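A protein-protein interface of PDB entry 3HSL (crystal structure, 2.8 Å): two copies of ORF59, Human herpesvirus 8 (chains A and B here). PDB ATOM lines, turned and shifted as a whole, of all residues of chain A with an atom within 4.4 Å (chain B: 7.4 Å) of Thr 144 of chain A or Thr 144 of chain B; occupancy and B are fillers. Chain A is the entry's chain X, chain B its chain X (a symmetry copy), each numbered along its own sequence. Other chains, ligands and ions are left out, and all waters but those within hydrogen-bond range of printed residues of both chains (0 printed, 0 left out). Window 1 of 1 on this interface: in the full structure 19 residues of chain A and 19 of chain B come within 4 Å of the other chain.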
ATOM      1  N   PHE A  97      16.647 -21.571  -9.809  1.00  0.00           N
ATOM      2  CA  PHE A  97      15.379 -20.891  -9.719  1.00  0.00           C
ATOM      3  C   PHE A  97      14.875 -20.635 -11.136  1.00  0.00           C
ATOM      4  O   PHE A  97      15.513 -19.940 -11.923  1.00  0.00           O
ATOM      5  CB  PHE A  97      15.360 -19.628  -8.874  1.00  0.00           C
ATOM      6  CG  PHE A  97      13.956 -19.136  -8.625  1.00  0.00           C
ATOM      7  CD1 PHE A  97      13.222 -19.615  -7.539  1.00  0.00           C
ATOM      8  CD2 PHE A  97      13.360 -18.210  -9.471  1.00  0.00           C
ATOM      9  CE1 PHE A  97      11.913 -19.168  -7.304  1.00  0.00           C
ATOM     10  CE2 PHE A  97      12.070 -17.758  -9.250  1.00  0.00           C
ATOM     11  CZ  PHE A  97      11.342 -18.234  -8.169  1.00  0.00           C
ATOM     12  N   THR A 133      10.197 -12.433  -6.965  1.00  0.00           N
ATOM     13  CA  THR A 133       9.122 -13.377  -7.127  1.00  0.00           C
ATOM     14  C   THR A 133       9.031 -14.037  -5.777  1.00  0.00           C
ATOM     15  O   THR A 133      10.031 -14.500  -5.209  1.00  0.00           O
ATOM     16  CB  THR A 133       9.396 -14.399  -8.244  1.00  0.00           C
ATOM     17  OG1 THR A 133       9.529 -13.707  -9.492  1.00  0.00           O
ATOM     18  CG2 THR A 133       8.264 -15.409  -8.354  1.00  0.00           C
ATOM     19  N   THR A 134       7.818 -14.068  -5.260  1.00  0.00           N
ATOM     20  CA  THR A 134       7.560 -14.670  -3.995  1.00  0.00           C
ATOM     21  C   THR A 134       6.662 -15.835  -4.260  1.00  0.00           C
ATOM     22  O   THR A 134       5.608 -15.659  -4.873  1.00  0.00           O
ATOM     23  CB  THR A 134       6.855 -13.686  -3.070  1.00  0.00           C
ATOM     24  OG1 THR A 134       7.776 -12.639  -2.748  1.00  0.00           O
ATOM     25  CG2 THR A 134       6.422 -14.368  -1.768  1.00  0.00           C
ATOM     26  N   ILE A 135       7.087 -17.011  -3.800  1.00  0.00           N
ATOM     27  CA  ILE A 135       6.294 -18.226  -3.931  1.00  0.00           C
ATOM     28  C   ILE A 135       5.931 -18.745  -2.510  1.00  0.00           C
ATOM     29  O   ILE A 135       6.778 -18.742  -1.598  1.00  0.00           O
ATOM     30  CB  ILE A 135       7.026 -19.338  -4.745  1.00  0.00           C
ATOM     31  CG1 ILE A 135       7.514 -18.841  -6.129  1.00  0.00           C
ATOM     32  CG2 ILE A 135       6.144 -20.574  -4.883  1.00  0.00           C
ATOM     33  CD1 ILE A 135       6.433 -18.361  -7.121  1.00  0.00           C
ATOM     34  N   TYR A 137       4.247 -22.104  -0.757  1.00  0.00           N
ATOM     35  CA  TYR A 137       3.909 -23.505  -0.977  1.00  0.00           C
ATOM     36  C   TYR A 137       2.716 -24.059  -0.190  1.00  0.00           C
ATOM     37  O   TYR A 137       2.194 -23.395   0.703  1.00  0.00           O
ATOM     38  CB  TYR A 137       5.192 -24.340  -0.807  1.00  0.00           C
ATOM     39  CG  TYR A 137       6.218 -23.896  -1.828  1.00  0.00           C
ATOM     40  CD1 TYR A 137       6.178 -24.386  -3.128  1.00  0.00           C
ATOM     41  CD2 TYR A 137       7.217 -22.984  -1.495  1.00  0.00           C
ATOM     42  CE1 TYR A 137       7.097 -23.991  -4.068  1.00  0.00           C
ATOM     43  CE2 TYR A 137       8.160 -22.570  -2.435  1.00  0.00           C
ATOM     44  CZ  TYR A 137       8.095 -23.078  -3.726  1.00  0.00           C
ATOM     45  OH  TYR A 137       9.017 -22.685  -4.687  1.00  0.00           O
ATOM     46  N   SER A 143       8.244 -21.018   1.861  1.00  0.00           N
ATOM     47  CA  SER A 143       8.247 -19.966   0.854  1.00  0.00           C
ATOM     48  C   SER A 143       9.646 -19.782   0.264  1.00  0.00           C
ATOM     49  O   SER A 143      10.638 -20.279   0.807  1.00  0.00           O
ATOM     50  CB  SER A 143       7.717 -18.627   1.403  1.00  0.00           C
ATOM     51  OG  SER A 143       8.606 -18.007   2.328  1.00  0.00           O
ATOM     52  N   THR A 144       9.705 -19.064  -0.855  1.00  0.00           N
ATOM     53  CA  THR A 144      10.952 -18.734  -1.539  1.00  0.00           C
ATOM     54  C   THR A 144      10.851 -17.294  -2.027  1.00  0.00           C
ATOM     55  O   THR A 144       9.814 -16.888  -2.565  1.00  0.00           O
ATOM     56  CB  THR A 144      11.196 -19.619  -2.766  1.00  0.00           C
ATOM     57  OG1 THR A 144      11.375 -20.996  -2.371  1.00  0.00           O
ATOM     58  CG2 THR A 144      12.438 -19.142  -3.518  1.00  0.00           C
ATOM     59  N   VAL A 145      11.906 -16.510  -1.841  1.00  0.00           N
ATOM     60  CA  VAL A 145      11.912 -15.125  -2.345  1.00  0.00           C
ATOM     61  C   VAL A 145      13.180 -14.945  -3.185  1.00  0.00           C
ATOM     62  O   VAL A 145      14.289 -14.838  -2.649  1.00  0.00           O
ATOM     63  CB  VAL A 145      11.783 -14.053  -1.247  1.00  0.00           C
ATOM     64  CG1 VAL A 145      11.938 -12.667  -1.842  1.00  0.00           C
ATOM     65  CG2 VAL A 145      10.443 -14.190  -0.525  1.00  0.00           C
ATOM     66  N   HIS A 146      12.990 -14.918  -4.501  1.00  0.00           N
ATOM     67  CA  HIS A 146      14.092 -14.786  -5.437  1.00  0.00           C
ATOM     68  C   HIS A 146      14.158 -13.394  -6.050  1.00  0.00           C
ATOM     69  O   HIS A 146      13.190 -12.941  -6.666  1.00  0.00           O
ATOM     70  CB  HIS A 146      13.952 -15.835  -6.547  1.00  0.00           C
ATOM     71  CG  HIS A 146      15.115 -15.881  -7.481  1.00  0.00           C
ATOM     72  ND1 HIS A 146      16.314 -16.470  -7.141  1.00  0.00           N
ATOM     73  CD2 HIS A 146      15.269 -15.419  -8.741  1.00  0.00           C
ATOM     74  CE1 HIS A 146      17.159 -16.369  -8.150  1.00  0.00           C
ATOM     75  NE2 HIS A 146      16.551 -15.736  -9.135  1.00  0.00           N
ATOM     76  N   SER B  92      12.427 -29.218   0.331  1.00  0.00           N
ATOM     77  CA  SER B  92      11.127 -28.999   0.970  1.00  0.00           C
ATOM     78  C   SER B  92      10.079 -29.544   0.031  1.00  0.00           C
ATOM     79  O   SER B  92      10.297 -29.515  -1.172  1.00  0.00           O
ATOM     80  CB  SER B  92      10.914 -27.505   1.118  1.00  0.00           C
ATOM     81  OG  SER B  92      12.034 -26.894   1.738  1.00  0.00           O
ATOM     82  N   SER B  95       8.647 -27.730  -3.402  1.00  0.00           N
ATOM     83  CA  SER B  95       9.735 -26.861  -3.863  1.00  0.00           C
ATOM     84  C   SER B  95      10.696 -27.335  -4.921  1.00  0.00           C
ATOM     85  O   SER B  95      10.819 -28.510  -5.271  1.00  0.00           O
ATOM     86  CB  SER B  95      10.601 -26.301  -2.702  1.00  0.00           C
ATOM     87  OG  SER B  95       9.949 -25.265  -1.996  1.00  0.00           O
ATOM     88  N   GLY B  96      11.366 -26.304  -5.394  1.00  0.00           N
ATOM     89  CA  GLY B  96      12.410 -26.340  -6.362  1.00  0.00           C
ATOM     90  C   GLY B  96      13.445 -25.546  -5.587  1.00  0.00           C
ATOM     91  O   GLY B  96      13.809 -24.397  -5.950  1.00  0.00           O
ATOM     92  N   PHE B  97      13.894 -26.178  -4.500  1.00  0.00           N
ATOM     93  CA  PHE B  97      14.939 -25.652  -3.658  1.00  0.00           C
ATOM     94  C   PHE B  97      15.612 -26.823  -2.947  1.00  0.00           C
ATOM     95  O   PHE B  97      14.980 -27.555  -2.189  1.00  0.00           O
ATOM     96  CB  PHE B  97      14.524 -24.560  -2.686  1.00  0.00           C
ATOM     97  CG  PHE B  97      15.714 -23.896  -2.041  1.00  0.00           C
ATOM     98  CD1 PHE B  97      16.337 -22.809  -2.659  1.00  0.00           C
ATOM     99  CD2 PHE B  97      16.224 -24.352  -0.832  1.00  0.00           C
ATOM    100  CE1 PHE B  97      17.448 -22.189  -2.069  1.00  0.00           C
ATOM    101  CE2 PHE B  97      17.319 -23.749  -0.239  1.00  0.00           C
ATOM    102  CZ  PHE B  97      17.935 -22.668  -0.853  1.00  0.00           C
ATOM    103  N   GLU B 102      22.308 -25.561  -3.793  1.00  0.00           N
ATOM    104  CA  GLU B 102      22.589 -24.132  -3.773  1.00  0.00           C
ATOM    105  C   GLU B 102      23.761 -23.791  -2.862  1.00  0.00           C
ATOM    106  O   GLU B 102      24.485 -22.837  -3.132  1.00  0.00           O
ATOM    107  CB  GLU B 102      21.356 -23.355  -3.314  1.00  0.00           C
ATOM    108  CG  GLU B 102      20.087 -23.686  -4.096  1.00  0.00           C
ATOM    109  CD  GLU B 102      20.234 -23.422  -5.575  1.00  0.00           C
ATOM    110  OE1 GLU B 102      20.792 -22.352  -5.934  1.00  0.00           O
ATOM    111  OE2 GLU B 102      19.790 -24.283  -6.380  1.00  0.00           O
ATOM    112  N   GLY B 112      24.066 -18.263   4.043  1.00  0.00           N
ATOM    113  CA  GLY B 112      23.834 -18.302   5.486  1.00  0.00           C
ATOM    114  C   GLY B 112      22.574 -19.075   5.804  1.00  0.00           C
ATOM    115  O   GLY B 112      21.665 -19.163   4.976  1.00  0.00           O
ATOM    116  N   ARG B 132      15.862 -20.547   7.518  1.00  0.00           N
ATOM    117  CA  ARG B 132      16.055 -19.626   6.399  1.00  0.00           C
ATOM    118  C   ARG B 132      17.439 -19.798   5.830  1.00  0.00           C
ATOM    119  O   ARG B 132      18.432 -19.788   6.571  1.00  0.00           O
ATOM    120  CB  ARG B 132      15.980 -18.146   6.705  1.00  0.00           C
ATOM    121  CG  ARG B 132      14.675 -17.417   6.651  1.00  0.00           C
ATOM    122  CD  ARG B 132      15.102 -15.949   6.458  1.00  0.00           C
ATOM    123  NE  ARG B 132      16.175 -15.611   7.408  1.00  0.00           N
ATOM    124  CZ  ARG B 132      16.874 -14.477   7.424  1.00  0.00           C
ATOM    125  NH1 ARG B 132      16.632 -13.530   6.530  1.00  0.00           N
ATOM    126  NH2 ARG B 132      17.824 -14.286   8.337  1.00  0.00           N
ATOM    127  N   THR B 133      17.510 -19.952   4.519  1.00  0.00           N
ATOM    128  CA  THR B 133      18.781 -20.078   3.857  1.00  0.00           C
ATOM    129  C   THR B 133      18.782 -18.927   2.885  1.00  0.00           C
ATOM    130  O   THR B 133      17.829 -18.720   2.119  1.00  0.00           O
ATOM    131  CB  THR B 133      18.946 -21.429   3.140  1.00  0.00           C
ATOM    132  OG1 THR B 133      18.880 -22.485   4.108  1.00  0.00           O
ATOM    133  CG2 THR B 133      20.279 -21.506   2.411  1.00  0.00           C
ATOM    134  N   THR B 134      19.861 -18.169   2.928  1.00  0.00           N
ATOM    135  CA  THR B 134      20.024 -17.050   2.064  1.00  0.00           C
ATOM    136  C   THR B 134      21.193 -17.361   1.189  1.00  0.00           C
ATOM    137  O   THR B 134      22.272 -17.664   1.703  1.00  0.00           O
ATOM    138  CB  THR B 134      20.315 -15.791   2.870  1.00  0.00           C
ATOM    139  OG1 THR B 134      19.140 -15.456   3.615  1.00  0.00           O
ATOM    140  CG2 THR B 134      20.657 -14.614   1.950  1.00  0.00           C
ATOM    141  N   ILE B 135      20.973 -17.288  -0.124  1.00  0.00           N
ATOM    142  CA  ILE B 135      22.030 -17.508  -1.101  1.00  0.00           C
ATOM    143  C   ILE B 135      22.247 -16.199  -1.911  1.00  0.00           C
ATOM    144  O   ILE B 135      21.276 -15.526  -2.301  1.00  0.00           O
ATOM    145  CB  ILE B 135      21.723 -18.698  -2.063  1.00  0.00           C
ATOM    146  CG1 ILE B 135      21.385 -20.007  -1.306  1.00  0.00           C
ATOM    147  CG2 ILE B 135      22.872 -18.909  -3.043  1.00  0.00           C
ATOM    148  CD1 ILE B 135      22.486 -20.593  -0.397  1.00  0.00           C
ATOM    149  N   SER B 136      23.518 -15.848  -2.150  1.00  0.00           N
ATOM    150  CA  SER B 136      23.890 -14.666  -2.912  1.00  0.00           C
ATOM    151  C   SER B 136      24.762 -15.164  -4.040  1.00  0.00           C
ATOM    152  O   SER B 136      25.811 -15.750  -3.798  1.00  0.00           O
ATOM    153  CB  SER B 136      24.655 -13.676  -2.047  1.00  0.00           C
ATOM    154  OG  SER B 136      23.868 -13.281  -0.942  1.00  0.00           O
ATOM    155  N   TYR B 137      24.315 -14.918  -5.269  1.00  0.00           N
ATOM    156  CA  TYR B 137      24.995 -15.369  -6.479  1.00  0.00           C
ATOM    157  C   TYR B 137      26.126 -14.478  -7.006  1.00  0.00           C
ATOM    158  O   TYR B 137      26.320 -13.363  -6.526  1.00  0.00           O
ATOM    159  CB  TYR B 137      23.923 -15.686  -7.539  1.00  0.00           C
ATOM    160  CG  TYR B 137      23.018 -16.785  -7.024  1.00  0.00           C
ATOM    161  CD1 TYR B 137      23.395 -18.119  -7.132  1.00  0.00           C
ATOM    162  CD2 TYR B 137      21.797 -16.489  -6.424  1.00  0.00           C
ATOM    163  CE1 TYR B 137      22.589 -19.128  -6.666  1.00  0.00           C
ATOM    164  CE2 TYR B 137      20.964 -17.499  -5.944  1.00  0.00           C
ATOM    165  CZ  TYR B 137      21.367 -18.823  -6.067  1.00  0.00           C
ATOM    166  OH  TYR B 137      20.562 -19.852  -5.597  1.00  0.00           O
ATOM    167  N   LEU B 141      24.254  -9.420  -7.427  1.00  0.00           N
ATOM    168  CA  LEU B 141      22.862  -8.937  -7.483  1.00  0.00           C
ATOM    169  C   LEU B 141      21.730  -9.952  -7.271  1.00  0.00           C
ATOM    170  O   LEU B 141      20.723  -9.617  -6.658  1.00  0.00           O
ATOM    171  CB  LEU B 141      22.632  -8.185  -8.824  1.00  0.00           C
ATOM    172  CG  LEU B 141      23.455  -6.924  -9.154  1.00  0.00           C
ATOM    173  CD1 LEU B 141      23.186  -6.448 -10.551  1.00  0.00           C
ATOM    174  CD2 LEU B 141      23.160  -5.808  -8.188  1.00  0.00           C
ATOM    175  N   THR B 142      21.893 -11.167  -7.775  1.00  0.00           N
ATOM    176  CA  THR B 142      20.869 -12.191  -7.637  1.00  0.00           C
ATOM    177  C   THR B 142      20.940 -12.912  -6.277  1.00  0.00           C
ATOM    178  O   THR B 142      22.029 -13.292  -5.811  1.00  0.00           O
ATOM    179  CB  THR B 142      21.010 -13.242  -8.781  1.00  0.00           C
ATOM    180  OG1 THR B 142      20.881 -12.595 -10.054  1.00  0.00           O
ATOM    181  CG2 THR B 142      19.976 -14.360  -8.678  1.00  0.00           C
ATOM    182  N   SER B 143      19.781 -13.097  -5.641  1.00  0.00           N
ATOM    183  CA  SER B 143      19.716 -13.813  -4.375  1.00  0.00           C
ATOM    184  C   SER B 143      18.437 -14.646  -4.287  1.00  0.00           C
ATOM    185  O   SER B 143      17.505 -14.469  -5.077  1.00  0.00           O
ATOM    186  CB  SER B 143      19.825 -12.869  -3.161  1.00  0.00           C
ATOM    187  OG  SER B 143      18.672 -12.053  -2.979  1.00  0.00           O
ATOM    188  N   THR B 144      18.414 -15.557  -3.316  1.00  0.00           N
ATOM    189  CA  THR B 144      17.264 -16.412  -3.038  1.00  0.00           C
ATOM    190  C   THR B 144      17.120 -16.524  -1.525  1.00  0.00           C
ATOM    191  O   THR B 144      18.116 -16.708  -0.815  1.00  0.00           O
ATOM    192  CB  THR B 144      17.445 -17.831  -3.590  1.00  0.00           C
ATOM    193  OG1 THR B 144      17.516 -17.810  -5.032  1.00  0.00           O
ATOM    194  CG2 THR B 144      16.278 -18.715  -3.153  1.00  0.00           C
ATOM    195  N   VAL B 145      15.899 -16.410  -1.017  1.00  0.00           N
ATOM    196  CA  VAL B 145      15.668 -16.575   0.430  1.00  0.00           C
ATOM    197  C   VAL B 145      14.559 -17.615   0.604  1.00  0.00           C
ATOM    198  O   VAL B 145      13.379 -17.335   0.367  1.00  0.00           O
ATOM    199  CB  VAL B 145      15.358 -15.262   1.172  1.00  0.00           C
ATOM    200  CG1 VAL B 145      14.999 -15.546   2.618  1.00  0.00           C
ATOM    201  CG2 VAL B 145      16.546 -14.305   1.083  1.00  0.00           C
ATOM    202  N   HIS B 146      14.966 -18.814   1.016  1.00  0.00           N
ATOM    203  CA  HIS B 146      14.043 -19.920   1.199  1.00  0.00           C
ATOM    204  C   HIS B 146      13.772 -20.200   2.671  1.00  0.00           C
ATOM    205  O   HIS B 146      14.704 -20.462   3.435  1.00  0.00           O
ATOM    206  CB  HIS B 146      14.608 -21.177   0.529  1.00  0.00           C
ATOM    207  CG  HIS B 146      13.668 -22.336   0.533  1.00  0.00           C
ATOM    208  ND1 HIS B 146      12.592 -22.419  -0.327  1.00  0.00           N
ATOM    209  CD2 HIS B 146      13.636 -23.460   1.282  1.00  0.00           C
ATOM    210  CE1 HIS B 146      11.936 -23.543  -0.107  1.00  0.00           C
ATOM    211  NE2 HIS B 146      12.548 -24.195   0.864  1.00  0.00           N
ATOM    212  N   LYS B 147      12.497 -20.141   3.051  1.00  0.00           N
ATOM    213  CA  LYS B 147      12.069 -20.421   4.412  1.00  0.00           C
ATOM    214  C   LYS B 147      11.402 -21.769   4.409  1.00  0.00           C
ATOM    215  O   LYS B 147      10.710 -22.124   3.447  1.00  0.00           O
ATOM    216  CB  LYS B 147      11.077 -19.375   4.929  1.00  0.00           C
ATOM    217  CG  LYS B 147      11.679 -17.990   5.017  1.00  0.00           C
ATOM    218  CD  LYS B 147      10.749 -16.938   5.602  1.00  0.00           C
ATOM    219  CE  LYS B 147      11.453 -15.572   5.604  1.00  0.00           C
ATOM    220  NZ  LYS B 147      10.644 -14.520   6.275  1.00  0.00           N
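The backbone carbonyl oxygen of Val 145 of chain B is in hydrogen-bond range of the backbone NH of Val 145 of chain A (2.8 Å).
The side-chain hydroxyl (OG1) of Thr 144 of chain A sits at hydrogen-bond distance from a ring nitrogen (ND1) of His 146 of chain B.
The backbone carbonyl oxygen (O) of Ser 143 of chain B is in hydrogen-bond range of a ring nitrogen (ND1) of His 146 of chain A, 3.1 Å away.
The backbone carbonyl oxygen of Ser 143 of chain A lies within hydrogen-bond range of the backbone NH of Lys 147 of chain B (2.9 Å).
O of Ser 143 of chain A sits at hydrogen-bond distance from ND1 of His 146 of chain B (3.1 Å).
A ring nitrogen (ND1) of His 146 of chain A sits at hydrogen-bond distance from the side-chain hydroxyl (OG1) of Thr 144 of chain B, 2.8 Å away.
The backbone NH (N) of Ile 135 of chain B sits at hydrogen-bond distance from the backbone carbonyl oxygen (O) of Thr 144 of chain B (3.0 Å).
The backbone NH (N) of Tyr 137 of chain B is in hydrogen-bond range of the backbone carbonyl oxygen (O) of Thr 142 of chain B (2.9 Å).
The backbone NH (N) of Thr 133 of chain A sits at hydrogen-bond distance from the backbone carbonyl oxygen (O) of His 146 of chain A (3.1 Å).
The side-chain hydroxyl (OG) of Ser 92 of chain B lies within hydrogen-bond range of a ring nitrogen (NE2) of His 146 of chain B, 2.9 Å away.
O of His 146 of chain B sits at hydrogen-bond distance from N of Thr 133 of chain B (3.1 Å).
N of Ile 135 of chain A sits at hydrogen-bond distance from O of Thr 144 of chain A, 3.0 Å away.
CE2 of Tyr 137 of chain A touches OG of Ser 95 of chain B, 3.3 Å away.
Thr 144 of chain B touches Thr 144 of chain A (CG2 to CG2, 3.9 Å).
Thr 144 of chain A touches Val 145 of chain B (CA to O, 3.4 Å).
O of Val 145 of chain A touches CA of Thr 144 of chain B, 3.4 Å away.
CE1 of His 146 of chain A touches CG2 of Thr 142 of chain B, 3.5 Å away.
Thr 144 of chain A touches just these residues of chain B: Thr 144 (3.9 Å), Val 145 (3.4 Å) and His 146 (2.8 Å).
Of the printed residues of chain B, Val 145 of chain A touches Thr 144 (3.4 Å) and Val 145 (2.8 Å).
Of the printed residues of chain B, His 146 of chain A touches Thr 142, Ser 143 and Thr 144.
Gly 112 of chain B touches none of the printed residues of chain A.
Arg 132 of chain B touches none of the printed residues of chain A.
Of the printed residues of chain A, Thr 142 of chain B touches His 146 (3.5 Å).
Of chain A, only Thr 144 (3.9 Å), Val 145 (3.4 Å) and His 146 (2.8 Å) come within 4 Å of Thr 144 of chain B.
Of the printed residues of chain A, His 146 of chain B touches Ser 143 and Thr 144.
Printed residues of chain A within 4 Å of Lys 147 of chain B: Ser 143.
The nearest printed residue of chain A that does not touch Val 145 of chain B is Ser 143 of chain A (4.05 Å).
Printed residues of chain A that touch a printed residue of chain B: Tyr 137, Ser 143, Thr 144, Val 145 and His 146.
Of the 19 printed residues of chain B, 7 touch a printed residue of chain A.
Hydrophobic or aromatic side chains of chain B that line the printed part of chain A: Val 145 and His 146.
Thr 144 of chain A touches its own counterpart, Thr 144 of chain B.
Thr 144 of chain A touches Val 145 of chain B, and with the chains exchanged Val 145 of chain A touches Thr 144 of chain B.
Thr 144 of chain A touches His 146 of chain B, and with the chains exchanged His 146 of chain A touches Thr 144 of chain B.
Val 145 of chain B touches its own counterpart, Val 145 of chain A.
9 positions are printed for both chains.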
